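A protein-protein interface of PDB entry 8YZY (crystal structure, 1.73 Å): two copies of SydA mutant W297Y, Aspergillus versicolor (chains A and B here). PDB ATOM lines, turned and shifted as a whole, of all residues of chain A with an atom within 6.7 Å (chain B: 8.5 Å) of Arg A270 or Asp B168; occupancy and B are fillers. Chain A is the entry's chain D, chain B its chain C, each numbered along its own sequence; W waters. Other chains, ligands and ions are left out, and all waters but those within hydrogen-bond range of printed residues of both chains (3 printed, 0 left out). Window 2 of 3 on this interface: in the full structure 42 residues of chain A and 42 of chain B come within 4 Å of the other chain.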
ATOM      1  N   SER A 263      25.345 -16.270  -4.420  1.00  0.00           N
ATOM      2  CA  SER A 263      24.479 -16.205  -3.244  1.00  0.00           C
ATOM      3  C   SER A 263      25.213 -15.571  -2.049  1.00  0.00           C
ATOM      4  O   SER A 263      24.615 -14.810  -1.270  1.00  0.00           O
ATOM      5  CB  SER A 263      23.960 -17.607  -2.927  1.00  0.00           C
ATOM      6  OG  SER A 263      23.490 -17.703  -1.598  1.00  0.00           O
ATOM      7  N   VAL A 265      27.646 -13.320  -2.323  1.00  0.00           N
ATOM      8  CA  VAL A 265      27.739 -11.900  -2.651  1.00  0.00           C
ATOM      9  C   VAL A 265      26.452 -11.183  -2.289  1.00  0.00           C
ATOM     10  O   VAL A 265      26.473 -10.110  -1.675  1.00  0.00           O
ATOM     11  CB  VAL A 265      28.060 -11.712  -4.139  1.00  0.00           C
ATOM     12  CG1 VAL A 265      27.867 -10.269  -4.556  1.00  0.00           C
ATOM     13  CG2 VAL A 265      29.518 -12.103  -4.368  1.00  0.00           C
ATOM     14  N   LEU A 266      25.312 -11.763  -2.683  1.00  0.00           N
ATOM     15  CA  LEU A 266      24.018 -11.165  -2.341  1.00  0.00           C
ATOM     16  C   LEU A 266      23.832 -11.068  -0.833  1.00  0.00           C
ATOM     17  O   LEU A 266      23.320 -10.055  -0.320  1.00  0.00           O
ATOM     18  CB  LEU A 266      22.888 -11.986  -2.939  1.00  0.00           C
ATOM     19  CG  LEU A 266      22.677 -11.866  -4.453  1.00  0.00           C
ATOM     20  CD1 LEU A 266      21.226 -12.134  -4.740  1.00  0.00           C
ATOM     21  CD2 LEU A 266      23.117 -10.483  -5.024  1.00  0.00           C
ATOM     22  N   GLU A 267      24.191 -12.127  -0.112  1.00  0.00           N
ATOM     23  CA  GLU A 267      24.062 -12.104   1.346  1.00  0.00           C
ATOM     24  C   GLU A 267      24.911 -10.990   1.966  1.00  0.00           C
ATOM     25  O   GLU A 267      24.438 -10.247   2.825  1.00  0.00           O
ATOM     26  CB  GLU A 267      24.448 -13.470   1.925  1.00  0.00           C
ATOM     27  CG  GLU A 267      24.929 -13.431   3.347  1.00  0.00           C
ATOM     28  CD  GLU A 267      25.330 -14.824   3.831  1.00  0.00           C
ATOM     29  OE1 GLU A 267      25.149 -15.152   5.022  1.00  0.00           O
ATOM     30  OE2 GLU A 267      25.786 -15.622   2.969  1.00  0.00           O
ATOM     31  N   ILE A 268      26.142 -10.820   1.506  1.00  0.00           N
ATOM     32  CA  ILE A 268      26.969  -9.734   2.026  1.00  0.00           C
ATOM     33  C   ILE A 268      26.383  -8.371   1.671  1.00  0.00           C
ATOM     34  O   ILE A 268      26.406  -7.439   2.489  1.00  0.00           O
ATOM     35  CB  ILE A 268      28.405  -9.880   1.499  1.00  0.00           C
ATOM     36  CG1 ILE A 268      29.092 -11.034   2.224  1.00  0.00           C
ATOM     37  CG2 ILE A 268      29.162  -8.576   1.701  1.00  0.00           C
ATOM     38  CD1 ILE A 268      30.422 -11.304   1.652  1.00  0.00           C
ATOM     39  N   HIS A 269      25.883  -8.214   0.437  1.00  0.00           N
ATOM     40  CA  HIS A 269      25.253  -6.943   0.084  1.00  0.00           C
ATOM     41  C   HIS A 269      24.072  -6.640   1.004  1.00  0.00           C
ATOM     42  O   HIS A 269      23.826  -5.481   1.342  1.00  0.00           O
ATOM     43  CB  HIS A 269      24.814  -6.943  -1.384  1.00  0.00           C
ATOM     44  CG  HIS A 269      25.952  -6.772  -2.344  1.00  0.00           C
ATOM     45  ND1 HIS A 269      25.785  -6.792  -3.714  1.00  0.00           N
ATOM     46  CD2 HIS A 269      27.277  -6.582  -2.128  1.00  0.00           C
ATOM     47  CE1 HIS A 269      26.957  -6.613  -4.301  1.00  0.00           C
ATOM     48  NE2 HIS A 269      27.877  -6.474  -3.362  1.00  0.00           N
ATOM     49  N   ARG A 270      23.323  -7.670   1.410  1.00  0.00           N
ATOM     50  CA  ARG A 270      22.182  -7.431   2.298  1.00  0.00           C
ATOM     51  C   ARG A 270      22.627  -7.088   3.724  1.00  0.00           C
ATOM     52  O   ARG A 270      22.141  -6.109   4.308  1.00  0.00           O
ATOM     53  CB  ARG A 270      21.271  -8.652   2.300  1.00  0.00           C
ATOM     54  CG  ARG A 270      20.532  -8.860   0.975  1.00  0.00           C
ATOM     55  CD  ARG A 270      19.741 -10.130   1.063  1.00  0.00           C
ATOM     56  NE  ARG A 270      19.161 -10.503  -0.213  1.00  0.00           N
ATOM     57  CZ  ARG A 270      19.418 -11.645  -0.824  1.00  0.00           C
ATOM     58  NH1 ARG A 270      20.261 -12.524  -0.308  1.00  0.00           N
ATOM     59  NH2 ARG A 270      18.816 -11.911  -1.980  1.00  0.00           N
ATOM     60  N   ILE A 271      23.513  -7.922   4.290  1.00  0.00           N
ATOM     61  CA  ILE A 271      24.031  -7.820   5.671  1.00  0.00           C
ATOM     62  C   ILE A 271      24.666  -6.465   5.933  1.00  0.00           C
ATOM     63  O   ILE A 271      24.550  -5.901   7.028  1.00  0.00           O
ATOM     64  CB  ILE A 271      25.098  -8.905   5.910  1.00  0.00           C
ATOM     65  CG1 ILE A 271      24.559 -10.314   5.912  1.00  0.00           C
ATOM     66  CG2 ILE A 271      25.905  -8.638   7.175  1.00  0.00           C
ATOM     67  CD1 ILE A 271      25.697 -11.251   6.280  1.00  0.00           C
ATOM     68  N   LEU A 272      25.478  -6.005   4.993  1.00  0.00           N
ATOM     69  CA  LEU A 272      26.219  -4.765   5.147  1.00  0.00           C
ATOM     70  C   LEU A 272      25.524  -3.578   4.478  1.00  0.00           C
ATOM     71  O   LEU A 272      26.113  -2.493   4.410  1.00  0.00           O
ATOM     72  CB  LEU A 272      27.639  -4.950   4.598  1.00  0.00           C
ATOM     73  CG  LEU A 272      28.509  -6.002   5.315  1.00  0.00           C
ATOM     74  CD1 LEU A 272      29.949  -6.101   4.744  1.00  0.00           C
ATOM     75  CD2 LEU A 272      28.528  -5.769   6.829  1.00  0.00           C
ATOM     76  N   ALA A 273      24.274  -3.737   4.029  1.00  0.00           N
ATOM     77  CA  ALA A 273      23.530  -2.591   3.512  1.00  0.00           C
ATOM     78  C   ALA A 273      23.554  -1.388   4.445  1.00  0.00           C
ATOM     79  O   ALA A 273      23.681  -0.258   3.940  1.00  0.00           O
ATOM     80  CB  ALA A 273      22.066  -2.961   3.197  1.00  0.00           C
ATOM     81  N   PRO A 274      23.403  -1.530   5.771  1.00  0.00           N
ATOM     82  CA  PRO A 274      23.413  -0.338   6.635  1.00  0.00           C
ATOM     83  C   PRO A 274      24.778   0.325   6.780  1.00  0.00           C
ATOM     84  O   PRO A 274      24.840   1.418   7.368  1.00  0.00           O
ATOM     85  CB  PRO A 274      22.935  -0.873   7.999  1.00  0.00           C
ATOM     86  CG  PRO A 274      22.372  -2.214   7.749  1.00  0.00           C
ATOM     87  CD  PRO A 274      23.048  -2.750   6.526  1.00  0.00           C
ATOM     88  N   LEU A 279      30.818  -2.314   3.483  1.00  0.00           N
ATOM     89  CA  LEU A 279      30.457  -2.905   2.204  1.00  0.00           C
ATOM     90  C   LEU A 279      31.457  -2.515   1.122  1.00  0.00           C
ATOM     91  O   LEU A 279      31.825  -3.352   0.287  1.00  0.00           O
ATOM     92  CB  LEU A 279      29.030  -2.497   1.799  1.00  0.00           C
ATOM     93  CG  LEU A 279      28.565  -3.171   0.488  1.00  0.00           C
ATOM     94  CD1 LEU A 279      28.713  -4.701   0.580  1.00  0.00           C
ATOM     95  CD2 LEU A 279      27.129  -2.791   0.155  1.00  0.00           C
ATOM     96  N   VAL B 165      21.412  -9.915  15.442  1.00  0.00           N
ATOM     97  CA  VAL B 165      21.613 -10.889  14.369  1.00  0.00           C
ATOM     98  C   VAL B 165      20.877 -10.388  13.124  1.00  0.00           C
ATOM     99  O   VAL B 165      19.652 -10.200  13.174  1.00  0.00           O
ATOM    100  CB  VAL B 165      21.166 -12.303  14.778  1.00  0.00           C
ATOM    101  CG1 VAL B 165      21.318 -13.257  13.630  1.00  0.00           C
ATOM    102  CG2 VAL B 165      22.073 -12.833  15.900  1.00  0.00           C
ATOM    103  N   PRO B 166      21.575 -10.109  12.029  1.00  0.00           N
ATOM    104  CA  PRO B 166      20.935  -9.452  10.875  1.00  0.00           C
ATOM    105  C   PRO B 166      19.965 -10.391  10.188  1.00  0.00           C
ATOM    106  O   PRO B 166      20.282 -11.571   9.968  1.00  0.00           O
ATOM    107  CB  PRO B 166      22.117  -9.121   9.944  1.00  0.00           C
ATOM    108  CG  PRO B 166      23.299  -9.180  10.796  1.00  0.00           C
ATOM    109  CD  PRO B 166      23.020 -10.275  11.809  1.00  0.00           C
ATOM    110  N   PRO B 167      18.798  -9.888   9.791  1.00  0.00           N
ATOM    111  CA  PRO B 167      17.774 -10.772   9.227  1.00  0.00           C
ATOM    112  C   PRO B 167      18.204 -11.622   8.044  1.00  0.00           C
ATOM    113  O   PRO B 167      17.674 -12.718   7.898  1.00  0.00           O
ATOM    114  CB  PRO B 167      16.663  -9.795   8.826  1.00  0.00           C
ATOM    115  CG  PRO B 167      16.798  -8.702   9.815  1.00  0.00           C
ATOM    116  CD  PRO B 167      18.276  -8.530  10.020  1.00  0.00           C
ATOM    117  N   ASP B 168      19.102 -11.192   7.178  1.00  0.00           N
ATOM    118  CA  ASP B 168      19.404 -12.040   6.023  1.00  0.00           C
ATOM    119  C   ASP B 168      20.780 -12.719   6.100  1.00  0.00           C
ATOM    120  O   ASP B 168      21.321 -13.149   5.070  1.00  0.00           O
ATOM    121  CB  ASP B 168      19.273 -11.217   4.748  1.00  0.00           C
ATOM    122  CG  ASP B 168      17.820 -10.852   4.438  1.00  0.00           C
ATOM    123  OD1 ASP B 168      16.937 -11.743   4.536  1.00  0.00           O
ATOM    124  OD2 ASP B 168      17.548  -9.686   4.082  1.00  0.00           O
ATOM    125  N   ALA B 169      21.352 -12.854   7.298  1.00  0.00           N
ATOM    126  CA  ALA B 169      22.700 -13.418   7.471  1.00  0.00           C
ATOM    127  C   ALA B 169      22.651 -14.950   7.557  1.00  0.00           C
ATOM    128  O   ALA B 169      22.862 -15.545   8.610  1.00  0.00           O
ATOM    129  CB  ALA B 169      23.363 -12.841   8.720  1.00  0.00           C
ATOM    130  N   LEU B 170      22.434 -15.602   6.402  1.00  0.00           N
ATOM    131  CA  LEU B 170      22.131 -17.036   6.375  1.00  0.00           C
ATOM    132  C   LEU B 170      23.273 -17.888   6.903  1.00  0.00           C
ATOM    133  O   LEU B 170      23.037 -18.908   7.559  1.00  0.00           O
ATOM    134  CB  LEU B 170      21.815 -17.479   4.949  1.00  0.00           C
ATOM    135  CG  LEU B 170      20.654 -16.734   4.348  1.00  0.00           C
ATOM    136  CD1 LEU B 170      20.368 -17.311   2.944  1.00  0.00           C
ATOM    137  CD2 LEU B 170      19.437 -16.850   5.263  1.00  0.00           C
ATOM    138  N   ARG B 171      24.512 -17.540   6.549  1.00  0.00           N
ATOM    139  CA  ARG B 171      25.675 -18.356   6.910  1.00  0.00           C
ATOM    140  C   ARG B 171      26.151 -18.108   8.328  1.00  0.00           C
ATOM    141  O   ARG B 171      26.890 -18.941   8.884  1.00  0.00           O
ATOM    142  CB  ARG B 171      26.798 -18.075   5.913  1.00  0.00           C
ATOM    143  CG  ARG B 171      26.999 -19.165   4.867  1.00  0.00           C
ATOM    144  CD  ARG B 171      25.758 -19.436   4.069  1.00  0.00           C
ATOM    145  NE  ARG B 171      25.439 -18.389   3.092  1.00  0.00           N
ATOM    146  CZ  ARG B 171      24.503 -18.511   2.152  1.00  0.00           C
ATOM    147  NH1 ARG B 171      23.744 -19.594   2.077  1.00  0.00           N
ATOM    148  NH2 ARG B 171      24.328 -17.527   1.260  1.00  0.00           N
ATOM    149  N   PHE B 172      25.738 -16.990   8.939  1.00  0.00           N
ATOM    150  CA  PHE B 172      26.298 -16.609  10.241  1.00  0.00           C
ATOM    151  C   PHE B 172      25.994 -17.615  11.348  1.00  0.00           C
ATOM    152  O   PHE B 172      26.917 -17.953  12.110  1.00  0.00           O
ATOM    153  CB  PHE B 172      25.809 -15.205  10.618  1.00  0.00           C
ATOM    154  CG  PHE B 172      26.339 -14.717  11.933  1.00  0.00           C
ATOM    155  CD1 PHE B 172      27.708 -14.682  12.177  1.00  0.00           C
ATOM    156  CD2 PHE B 172      25.468 -14.346  12.932  1.00  0.00           C
ATOM    157  CE1 PHE B 172      28.207 -14.256  13.408  1.00  0.00           C
ATOM    158  CE2 PHE B 172      25.948 -13.919  14.156  1.00  0.00           C
ATOM    159  CZ  PHE B 172      27.320 -13.877  14.396  1.00  0.00           C
ATOM    160  N   PRO B 173      24.752 -18.115  11.523  1.00  0.00           N
ATOM    161  CA  PRO B 173      24.513 -19.048  12.638  1.00  0.00           C
ATOM    162  C   PRO B 173      25.461 -20.231  12.662  1.00  0.00           C
ATOM    163  O   PRO B 173      25.972 -20.606  13.744  1.00  0.00           O
ATOM    164  CB  PRO B 173      23.061 -19.499  12.405  1.00  0.00           C
ATOM    165  CG  PRO B 173      22.426 -18.301  11.684  1.00  0.00           C
ATOM    166  CD  PRO B 173      23.503 -17.771  10.800  1.00  0.00           C
ATOM    167  N   ASN B 241      19.387 -18.347  16.287  1.00  0.00           N
ATOM    168  CA  ASN B 241      20.039 -17.556  15.246  1.00  0.00           C
ATOM    169  C   ASN B 241      19.511 -17.927  13.872  1.00  0.00           C
ATOM    170  O   ASN B 241      19.325 -17.050  13.020  1.00  0.00           O
ATOM    171  CB  ASN B 241      21.569 -17.724  15.310  1.00  0.00           C
ATOM    172  CG  ASN B 241      22.195 -17.031  16.537  1.00  0.00           C
ATOM    173  OD1 ASN B 241      21.591 -16.144  17.158  1.00  0.00           O
ATOM    174  ND2 ASN B 241      23.392 -17.460  16.904  1.00  0.00           N
ATOM    175  N   ASN B 244      16.092 -16.272  13.489  1.00  0.00           N
ATOM    176  CA  ASN B 244      16.136 -14.830  13.256  1.00  0.00           C
ATOM    177  C   ASN B 244      16.708 -14.486  11.883  1.00  0.00           C
ATOM    178  O   ASN B 244      16.291 -13.495  11.277  1.00  0.00           O
ATOM    179  CB  ASN B 244      16.953 -14.138  14.340  1.00  0.00           C
ATOM    180  CG  ASN B 244      16.143 -13.888  15.598  1.00  0.00           C
ATOM    181  OD1 ASN B 244      14.957 -13.541  15.535  1.00  0.00           O
ATOM    182  ND2 ASN B 244      16.769 -14.099  16.753  1.00  0.00           N
ATOM    183  N   THR B 245      17.673 -15.260  11.389  1.00  0.00           N
ATOM    184  CA  THR B 245      18.214 -14.991  10.060  1.00  0.00           C
ATOM    185  C   THR B 245      17.309 -15.469   8.932  1.00  0.00           C
ATOM    186  O   THR B 245      17.484 -15.047   7.780  1.00  0.00           O
ATOM    187  CB  THR B 245      19.564 -15.668   9.885  1.00  0.00           C
ATOM    188  OG1 THR B 245      19.416 -17.076  10.098  1.00  0.00           O
ATOM    189  CG2 THR B 245      20.592 -15.090  10.827  1.00  0.00           C
ATOM    190  N   THR B 246      16.401 -16.392   9.199  1.00  0.00           N
ATOM    191  CA  THR B 246      15.519 -16.861   8.141  1.00  0.00           C
ATOM    192  C   THR B 246      14.091 -16.350   8.311  1.00  0.00           C
ATOM    193  O   THR B 246      13.246 -16.654   7.464  1.00  0.00           O
ATOM    194  CB  THR B 246      15.538 -18.403   8.066  1.00  0.00           C
ATOM    195  OG1 THR B 246      15.007 -18.939   9.281  1.00  0.00           O
ATOM    196  CG2 THR B 246      16.991 -18.874   7.944  1.00  0.00           C
ATOM    197  N   GLY B 247      13.800 -15.597   9.383  1.00  0.00           N
ATOM    198  CA  GLY B 247      12.454 -15.112   9.634  1.00  0.00           C
ATOM    199  C   GLY B 247      11.466 -16.211   9.910  1.00  0.00           C
ATOM    200  O   GLY B 247      10.267 -16.033   9.692  1.00  0.00           O
HETATM  201  O   HOH W   1      21.591 -19.317  -0.265  1.00  0.00           O
HETATM  202  O   HOH W   2      25.911 -14.535   7.258  1.00  0.00           O
HETATM  203  O   HOH W   3      20.741 -13.559   2.329  1.00  0.00           O
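Among the printed residues, merely in contact across the chains: Glu A267 with Ala B169 (3.6 Å), Arg A270 with Asp B168 (3.8 Å) and Ile A271 with Ala B169 (3.7 Å).
No position is printed for both chains.
Water W2 lies within hydrogen-bond range of the side-chain carboxylate of Glu A267 (2.4 Å), the backbone NH of Phe B172 (3.0 Å), the backbone NH of Arg B171 (3.4 Å) and the backbone carbonyl oxygen of Ala B169 (3.5 Å). Water W1 lies within hydrogen-bond range of OG of Ser A263 (2.8 Å) and NH1 of Arg B171 (3.2 Å). Water W3 bridges O of Asp B168 (2.8 Å) and NH1 of Arg A270 (2.9 Å).
OE1 of Glu A267 is in hydrogen-bond range of N of Leu B170, at 3.1 Å. The guanidinium group (NH2) of Arg B171 sits at hydrogen-bond distance from the side-chain hydroxyl (OG) of Ser A263 (3.0 Å). NE of Arg B171 lies within salt-bridge range of OE2 of Glu A267, at 2.8 Å.
Of the 14 printed residues of chain B, 4 touch a printed residue of chain A. Hydrophobic or aromatic side chains of chain B that line the printed part of chain A: Ala B169. Among the printed residues, 6 pairs touch across the chains. Among the printed residues, Asp or Glu carboxylates within 4 Å of a Lys or Arg side-chain nitrogen of the other chain: Glu A267 with Arg B171 (2.8 Å).
Of chain B, only Asp B168 (3.8 Å) comes within 4 Å of Arg A270. Of the printed residues of chain A, Ala B169 touches Glu A267 (3.6 Å) and Ile A271 (3.7 Å). Of the printed residues of chain A, Leu B170 touches Glu A267. Of the printed residues of chain B, Ser A263 touches Arg B171 (3.0 Å). The nearest residue of chain B that does not touch Arg A270 is Leu B170 (5.8 Å).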
